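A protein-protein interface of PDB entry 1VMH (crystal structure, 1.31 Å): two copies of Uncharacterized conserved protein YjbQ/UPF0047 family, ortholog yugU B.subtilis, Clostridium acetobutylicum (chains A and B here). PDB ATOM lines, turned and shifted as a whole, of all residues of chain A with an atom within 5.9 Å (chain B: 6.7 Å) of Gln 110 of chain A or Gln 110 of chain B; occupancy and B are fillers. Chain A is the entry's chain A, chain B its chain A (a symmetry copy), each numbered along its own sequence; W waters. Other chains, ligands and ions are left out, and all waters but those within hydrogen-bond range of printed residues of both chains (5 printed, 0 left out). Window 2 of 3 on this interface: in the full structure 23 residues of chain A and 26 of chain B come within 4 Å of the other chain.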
ATOM      1  N   MET A  49      23.166   5.898  26.199  1.00  0.00           N
ATOM      2  CA  MET A  49      21.742   6.107  26.171  1.00  0.00           C
ATOM      3  C   MET A  49      21.014   4.852  26.615  1.00  0.00           C
ATOM      4  O   MET A  49      21.423   3.733  26.302  1.00  0.00           O
ATOM      5  CB  MET A  49      21.311   6.410  24.715  1.00  0.00           C
ATOM      6  CG  MET A  49      21.764   7.727  24.151  1.00  0.00           C
ATOM      7  SD  MET A  49      21.224   9.192  25.055  1.00  0.00           S
ATOM      8  CE  MET A  49      19.476   8.968  25.041  1.00  0.00           C
ATOM      9  N   ALA A  50      19.910   5.050  27.320  1.00  0.00           N
ATOM     10  CA  ALA A  50      18.979   3.956  27.615  1.00  0.00           C
ATOM     11  C   ALA A  50      17.746   4.164  26.772  1.00  0.00           C
ATOM     12  O   ALA A  50      17.147   5.250  26.799  1.00  0.00           O
ATOM     13  CB  ALA A  50      18.593   4.010  29.064  1.00  0.00           C
ATOM     14  N   VAL A  51      17.357   3.138  26.018  1.00  0.00           N
ATOM     15  CA  VAL A  51      16.153   3.182  25.196  1.00  0.00           C
ATOM     16  C   VAL A  51      15.147   2.223  25.782  1.00  0.00           C
ATOM     17  O   VAL A  51      15.526   1.080  26.091  1.00  0.00           O
ATOM     18  CB  VAL A  51      16.483   2.770  23.726  1.00  0.00           C
ATOM     19  CG1 VAL A  51      15.208   2.764  22.892  1.00  0.00           C
ATOM     20  CG2 VAL A  51      17.507   3.722  23.119  1.00  0.00           C
ATOM     21  N   VAL A  52      13.913   2.697  26.017  1.00  0.00           N
ATOM     22  CA  VAL A  52      12.869   1.961  26.652  1.00  0.00           C
ATOM     23  C   VAL A  52      11.714   1.851  25.659  1.00  0.00           C
ATOM     24  O   VAL A  52      11.187   2.873  25.266  1.00  0.00           O
ATOM     25  CB  VAL A  52      12.377   2.686  27.925  1.00  0.00           C
ATOM     26  CG1 VAL A  52      11.312   1.900  28.641  1.00  0.00           C
ATOM     27  CG2 VAL A  52      13.555   2.960  28.865  1.00  0.00           C
ATOM     28  N   PHE A  53      11.371   0.657  25.223  1.00  0.00           N
ATOM     29  CA  PHE A  53      10.420   0.435  24.111  1.00  0.00           C
ATOM     30  C   PHE A  53       9.231  -0.445  24.557  1.00  0.00           C
ATOM     31  O   PHE A  53       9.433  -1.501  25.211  1.00  0.00           O
ATOM     32  CB  PHE A  53      11.136  -0.248  22.935  1.00  0.00           C
ATOM     33  CG  PHE A  53      10.300  -0.377  21.675  1.00  0.00           C
ATOM     34  CD1 PHE A  53       9.464  -1.477  21.488  1.00  0.00           C
ATOM     35  CD2 PHE A  53      10.356   0.588  20.685  1.00  0.00           C
ATOM     36  CE1 PHE A  53       8.713  -1.576  20.336  1.00  0.00           C
ATOM     37  CE2 PHE A  53       9.586   0.479  19.560  1.00  0.00           C
ATOM     38  CZ  PHE A  53       8.761  -0.569  19.400  1.00  0.00           C
ATOM     39  N   ILE A  63       7.706   9.985  30.246  1.00  0.00           N
ATOM     40  CA  ILE A  63       8.573  10.412  31.392  1.00  0.00           C
ATOM     41  C   ILE A  63       7.845  11.562  32.034  1.00  0.00           C
ATOM     42  O   ILE A  63       7.486  12.510  31.330  1.00  0.00           O
ATOM     43  CB  ILE A  63       9.975  10.790  30.897  1.00  0.00           C
ATOM     44  CG1 ILE A  63      10.661   9.552  30.279  1.00  0.00           C
ATOM     45  CG2 ILE A  63      10.828  11.384  31.996  1.00  0.00           C
ATOM     46  CD1 ILE A  63      12.084   9.715  29.757  1.00  0.00           C
ATOM     47  N   SER A 107       5.762   5.180  21.681  1.00  0.00           N
ATOM     48  CA  SER A 107       6.169   3.779  21.732  1.00  0.00           C
ATOM     49  C   SER A 107       7.504   3.572  22.438  1.00  0.00           C
ATOM     50  O   SER A 107       7.768   2.463  22.897  1.00  0.00           O
ATOM     51  CB  SER A 107       6.239   3.210  20.304  1.00  0.00           C
ATOM     52  OG  SER A 107       7.110   4.004  19.480  1.00  0.00           O
ATOM     53  N   SER A 108       8.288   4.625  22.622  1.00  0.00           N
ATOM     54  CA  SER A 108       9.561   4.537  23.330  1.00  0.00           C
ATOM     55  C   SER A 108       9.939   5.879  23.888  1.00  0.00           C
ATOM     56  O   SER A 108       9.433   6.933  23.472  1.00  0.00           O
ATOM     57  CB  SER A 108      10.669   4.042  22.397  1.00  0.00           C
ATOM     58  OG  SER A 108      11.034   5.044  21.454  1.00  0.00           O
ATOM     59  N   GLN A 109      10.816   5.836  24.872  1.00  0.00           N
ATOM     60  CA  GLN A 109      11.512   7.017  25.303  1.00  0.00           C
ATOM     61  C   GLN A 109      12.987   6.653  25.503  1.00  0.00           C
ATOM     62  O   GLN A 109      13.382   5.478  25.665  1.00  0.00           O
ATOM     63  CB  GLN A 109      10.909   7.619  26.564  1.00  0.00           C
ATOM     64  CG  GLN A 109       9.426   7.955  26.457  1.00  0.00           C
ATOM     65  CD  GLN A 109       9.110   9.034  25.472  1.00  0.00           C
ATOM     66  OE1 GLN A 109       9.984   9.799  25.056  1.00  0.00           O
ATOM     67  NE2 GLN A 109       7.820   9.146  25.113  1.00  0.00           N
ATOM     68  N   GLN A 110      13.812   7.688  25.595  1.00  0.00           N
ATOM     69  CA  GLN A 110      15.245   7.494  25.802  1.00  0.00           C
ATOM     70  C   GLN A 110      15.774   8.483  26.817  1.00  0.00           C
ATOM     71  O   GLN A 110      15.240   9.593  26.977  1.00  0.00           O
ATOM     72  CB  GLN A 110      16.037   7.434  24.507  1.00  0.00           C
ATOM     73  CG  GLN A 110      16.059   8.656  23.697  1.00  0.00           C
ATOM     74  CD  GLN A 110      16.939   8.475  22.448  1.00  0.00           C
ATOM     75  OE1 GLN A 110      17.807   7.545  22.344  1.00  0.00           O
ATOM     76  NE2 GLN A 110      16.687   9.316  21.490  1.00  0.00           N
ATOM     77  N   ILE A 111      16.784   8.027  27.565  1.00  0.00           N
ATOM     78  CA  ILE A 111      17.338   8.772  28.674  1.00  0.00           C
ATOM     79  C   ILE A 111      18.863   8.713  28.546  1.00  0.00           C
ATOM     80  O   ILE A 111      19.449   7.669  28.259  1.00  0.00           O
ATOM     81  CB  ILE A 111      16.877   8.166  30.019  1.00  0.00           C
ATOM     82  CG1 ILE A 111      15.346   8.016  30.062  1.00  0.00           C
ATOM     83  CG2 ILE A 111      17.384   9.001  31.207  1.00  0.00           C
ATOM     84  CD1 ILE A 111      14.836   6.678  29.571  1.00  0.00           C
ATOM     85  N   ILE A 112      19.509   9.836  28.794  1.00  0.00           N
ATOM     86  CA  ILE A 112      20.945   9.916  28.767  1.00  0.00           C
ATOM     87  C   ILE A 112      21.492   9.203  29.983  1.00  0.00           C
ATOM     88  O   ILE A 112      20.931   9.305  31.105  1.00  0.00           O
ATOM     89  CB  ILE A 112      21.386  11.366  28.776  1.00  0.00           C
ATOM     90  CG1 ILE A 112      20.956  12.053  27.467  1.00  0.00           C
ATOM     91  CG2 ILE A 112      22.910  11.486  28.929  1.00  0.00           C
ATOM     92  CD1 ILE A 112      20.857  13.622  27.563  1.00  0.00           C
ATOM     93  N   MET B  49      19.935   0.059  16.463  1.00  0.00           N
ATOM     94  CA  MET B  49      18.713   0.819  16.455  1.00  0.00           C
ATOM     95  C   MET B  49      18.404   1.309  15.051  1.00  0.00           C
ATOM     96  O   MET B  49      19.302   1.681  14.294  1.00  0.00           O
ATOM     97  CB  MET B  49      18.894   2.065  17.357  1.00  0.00           C
ATOM     98  CG  MET B  49      19.008   1.801  18.833  1.00  0.00           C
ATOM     99  SD  MET B  49      17.611   0.944  19.586  1.00  0.00           S
ATOM    100  CE  MET B  49      16.285   2.019  19.150  1.00  0.00           C
ATOM    101  N   ALA B  50      17.120   1.339  14.725  1.00  0.00           N
ATOM    102  CA  ALA B  50      16.651   2.003  13.505  1.00  0.00           C
ATOM    103  C   ALA B  50      15.946   3.271  13.916  1.00  0.00           C
ATOM    104  O   ALA B  50      15.035   3.234  14.757  1.00  0.00           O
ATOM    105  CB  ALA B  50      15.676   1.110  12.798  1.00  0.00           C
ATOM    106  N   VAL B  51      16.357   4.398  13.338  1.00  0.00           N
ATOM    107  CA  VAL B  51      15.728   5.688  13.601  1.00  0.00           C
ATOM    108  C   VAL B  51      15.018   6.131  12.347  1.00  0.00           C
ATOM    109  O   VAL B  51      15.624   6.057  11.263  1.00  0.00           O
ATOM    110  CB  VAL B  51      16.805   6.746  14.002  1.00  0.00           C
ATOM    111  CG1 VAL B  51      16.143   8.101  14.219  1.00  0.00           C
ATOM    112  CG2 VAL B  51      17.541   6.310  15.264  1.00  0.00           C
ATOM    113  N   VAL B  52      13.732   6.497  12.468  1.00  0.00           N
ATOM    114  CA  VAL B  52      12.884   6.853  11.377  1.00  0.00           C
ATOM    115  C   VAL B  52      12.429   8.293  11.596  1.00  0.00           C
ATOM    116  O   VAL B  52      11.787   8.554  12.593  1.00  0.00           O
ATOM    117  CB  VAL B  52      11.644   5.932  11.318  1.00  0.00           C
ATOM    118  CG1 VAL B  52      10.763   6.254  10.141  1.00  0.00           C
ATOM    119  CG2 VAL B  52      12.078   4.464  11.269  1.00  0.00           C
ATOM    120  N   ILE B  61       5.680  10.481  12.545  1.00  0.00           N
ATOM    121  CA  ILE B  61       5.919   9.030  12.575  1.00  0.00           C
ATOM    122  C   ILE B  61       5.290   8.477  13.840  1.00  0.00           C
ATOM    123  O   ILE B  61       5.432   9.066  14.908  1.00  0.00           O
ATOM    124  CB  ILE B  61       7.424   8.678  12.597  1.00  0.00           C
ATOM    125  CG1 ILE B  61       8.193   9.404  11.473  1.00  0.00           C
ATOM    126  CG2 ILE B  61       7.631   7.174  12.552  1.00  0.00           C
ATOM    127  CD1 ILE B  61       7.923   8.997  10.050  1.00  0.00           C
ATOM    128  N   ILE B  63       4.042   4.433  15.840  1.00  0.00           N
ATOM    129  CA  ILE B  63       4.074   2.935  15.780  1.00  0.00           C
ATOM    130  C   ILE B  63       2.761   2.486  16.360  1.00  0.00           C
ATOM    131  O   ILE B  63       2.420   2.911  17.467  1.00  0.00           O
ATOM    132  CB  ILE B  63       5.287   2.390  16.545  1.00  0.00           C
ATOM    133  CG1 ILE B  63       6.590   2.874  15.871  1.00  0.00           C
ATOM    134  CG2 ILE B  63       5.265   0.880  16.649  1.00  0.00           C
ATOM    135  CD1 ILE B  63       7.913   2.406  16.466  1.00  0.00           C
ATOM    136  N   SER B 108       9.940  11.620  14.971  1.00  0.00           N
ATOM    137  CA  SER B 108      10.692  10.392  14.735  1.00  0.00           C
ATOM    138  C   SER B 108      10.240   9.315  15.679  1.00  0.00           C
ATOM    139  O   SER B 108       9.612   9.570  16.719  1.00  0.00           O
ATOM    140  CB  SER B 108      12.194  10.629  14.915  1.00  0.00           C
ATOM    141  OG  SER B 108      12.526  10.806  16.289  1.00  0.00           O
ATOM    142  N   GLN B 109      10.530   8.088  15.292  1.00  0.00           N
ATOM    143  CA  GLN B 109      10.454   6.981  16.202  1.00  0.00           C
ATOM    144  C   GLN B 109      11.700   6.111  16.002  1.00  0.00           C
ATOM    145  O   GLN B 109      12.396   6.151  14.965  1.00  0.00           O
ATOM    146  CB  GLN B 109       9.175   6.173  16.029  1.00  0.00           C
ATOM    147  CG  GLN B 109       7.892   6.984  16.160  1.00  0.00           C
ATOM    148  CD  GLN B 109       7.661   7.553  17.523  1.00  0.00           C
ATOM    149  OE1 GLN B 109       8.263   7.120  18.509  1.00  0.00           O
ATOM    150  NE2 GLN B 109       6.732   8.520  17.609  1.00  0.00           N
ATOM    151  N   GLN B 110      11.934   5.235  16.969  1.00  0.00           N
ATOM    152  CA  GLN B 110      13.078   4.329  16.906  1.00  0.00           C
ATOM    153  C   GLN B 110      12.679   2.938  17.346  1.00  0.00           C
ATOM    154  O   GLN B 110      11.752   2.755  18.153  1.00  0.00           O
ATOM    155  CB  GLN B 110      14.318   4.877  17.592  1.00  0.00           C
ATOM    156  CG  GLN B 110      14.228   5.075  19.041  1.00  0.00           C
ATOM    157  CD  GLN B 110      15.565   5.578  19.614  1.00  0.00           C
ATOM    158  OE1 GLN B 110      16.671   5.470  18.984  1.00  0.00           O
ATOM    159  NE2 GLN B 110      15.466   6.170  20.767  1.00  0.00           N
ATOM    160  N   ILE B 111      13.341   1.949  16.734  1.00  0.00           N
ATOM    161  CA  ILE B 111      13.014   0.553  16.922  1.00  0.00           C
ATOM    162  C   ILE B 111      14.330  -0.197  17.150  1.00  0.00           C
ATOM    163  O   ILE B 111      15.332   0.031  16.469  1.00  0.00           O
ATOM    164  CB  ILE B 111      12.275  -0.002  15.684  1.00  0.00           C
ATOM    165  CG1 ILE B 111      11.072   0.883  15.315  1.00  0.00           C
ATOM    166  CG2 ILE B 111      11.841  -1.461  15.904  1.00  0.00           C
ATOM    167  CD1 ILE B 111      11.386   1.983  14.323  1.00  0.00           C
ATOM    168  N   ILE B 112      14.316  -1.119  18.093  1.00  0.00           N
ATOM    169  CA  ILE B 112      15.462  -1.938  18.379  1.00  0.00           C
ATOM    170  C   ILE B 112      15.639  -2.933  17.254  1.00  0.00           C
ATOM    171  O   ILE B 112      14.647  -3.496  16.721  1.00  0.00           O
ATOM    172  CB  ILE B 112      15.263  -2.672  19.691  1.00  0.00           C
ATOM    173  CG1 ILE B 112      15.233  -1.666  20.855  1.00  0.00           C
ATOM    174  CG2 ILE B 112      16.385  -3.692  19.938  1.00  0.00           C
ATOM    175  CD1 ILE B 112      14.511  -2.198  22.151  1.00  0.00           C
ATOM    176  N   ILE B 144      21.871   2.506  13.156  1.00  0.00           N
ATOM    177  CA  ILE B 144      23.063   2.691  13.972  1.00  0.00           C
ATOM    178  C   ILE B 144      23.377   1.376  14.688  1.00  0.00           C
ATOM    179  O   ILE B 144      22.547   0.895  15.445  1.00  0.00           O
ATOM    180  CB  ILE B 144      22.841   3.816  14.988  1.00  0.00           C
ATOM    181  CG1 ILE B 144      22.349   5.088  14.281  1.00  0.00           C
ATOM    182  CG2 ILE B 144      24.153   4.137  15.729  1.00  0.00           C
ATOM    183  CD1 ILE B 144      21.290   5.823  15.038  1.00  0.00           C
ATOM    184  OXT ILE B 144      24.429   0.745  14.510  1.00  0.00           O
HETATM  185  O   HOH W   1      12.905   6.843  21.955  1.00  0.00           O
HETATM  186  O   HOH W   2       5.111   5.900  18.669  1.00  0.00           O
HETATM  187  O   HOH W   3      10.996   7.671  19.494  1.00  0.00           O
HETATM  188  O   HOH W   4       7.778   7.463  21.160  1.00  0.00           O
HETATM  189  O   HOH W   5       9.798   4.492  19.207  1.00  0.00           O
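Met 49 of chain B touches Val 51 of chain A. Gln 110 of chain B touches Val 51 of chain A (NE2 to CG2, 3.96 Å). Phe 53 of chain A touches Gln 110 of chain B. Ile 112 of chain B touches Phe 53 of chain A. CD1 of Ile 63 of chain B touches OG of Ser 107 of chain A, 3.5 Å away.
Val 51 of chain A touches Met 49 of chain B, but with the chains exchanged Met 49 of chain A does not touch Val 51 of chain B (9.9 Å). Val 51 of chain A touches Gln 110 of chain B, but with the chains exchanged Gln 110 of chain A does not touch Val 51 of chain B (7.0 Å). Gln 110 of chain A touches its own counterpart, Gln 110 of chain B. Positions printed for both chains: 49, 50, 51, 52, 63, 108, 109, 110, 111 and 112.
Printed residues of chain B within 4 Å of Val 51 of chain A: Met 49 and Gln 110. Printed residues of chain B within 4 Å of Phe 53 of chain A: Gln 110 and Ile 112. Of the printed residues of chain B, Ser 107 of chain A touches Ile 63 (3.5 Å) and Gln 109 (3.5 Å). Printed residues of chain A within 4 Å of Gln 109 of chain B: Ser 107. Of the printed residues of chain A, Gln 110 of chain B touches Val 51 (3.96 Å), Phe 53 (3.4 Å) and Gln 110 (3.1 Å). The nearest residue of chain B that does not touch Gln 110 of chain A is Met 49 of chain B (6.6 Å). The nearest printed residue of chain A that does not touch Gln 110 of chain B is Ser 108 of chain A (4.003 Å). The nearest printed residue of chain A that does not touch Ile 112 of chain B is Val 51 of chain A (4.9 Å).
OE1 of Gln 109 of chain B is in hydrogen-bond range of OG of Ser 107 of chain A (3.5 Å). OE1 of Gln 110 of chain A is in hydrogen-bond range of NE2 of Gln 110 of chain B.
The backbone NH (N) of Met 49 of chain B lies within hydrogen-bond range of the chain-end carboxylate (O) of Ile 144 of chain B. O of Ile 61 of chain B lies within hydrogen-bond range of NE2 of Gln 109 of chain B, at 3.0 Å. The backbone NH (N) of Val 52 of chain B lies within hydrogen-bond range of the backbone carbonyl oxygen (O) of Gln 109 of chain B.
Water W5 lies within hydrogen-bond range of OG of Ser 108 of chain A (2.6 Å), OG of Ser 107 of chain A (2.7 Å), O of Gln 110 of chain B (2.8 Å) and OE1 of Gln 109 of chain B (3.1 Å). Water W1 lies within hydrogen-bond range of OG of Ser 108 of chain A (2.6 Å) and NE2 of Gln 110 of chain B (2.9 Å). Water W4 lies within hydrogen-bond range of OE1 of Gln 109 of chain B (2.7 Å), O of Ser 108 of chain A (2.9 Å) and N of Ser 107 of chain A (3.1 Å). Water W2 lies within hydrogen-bond range of OG of Ser 107 of chain A, NE2 of Gln 109 of chain B and N of Ile 63 of chain B. Water W3 bridges OE1 of Gln 109 of chain B (3.0 Å) and OG of Ser 108 of chain A (3.3 Å).
Of the 12 printed residues of chain B, 5 touch a printed residue of chain A. Printed residues of chain B that touch a printed residue of chain A: Met 49, Ile 63, Gln 109, Gln 110 and Ile 112. Hydrophobic or aromatic side chains of chain B that line the printed part of chain A: Met 49, Ile 63 and Ile 112. Of the 12 printed residues of chain A, 4 touch a printed residue of chain B. Hydrophobic or aromatic side chains of chain A that line the printed part of chain B: Val 51 and Phe 53. Among the printed residues, no Asp or Glu carboxylate lies within 4 Å of a Lys or Arg side-chain nitrogen of the other chain.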
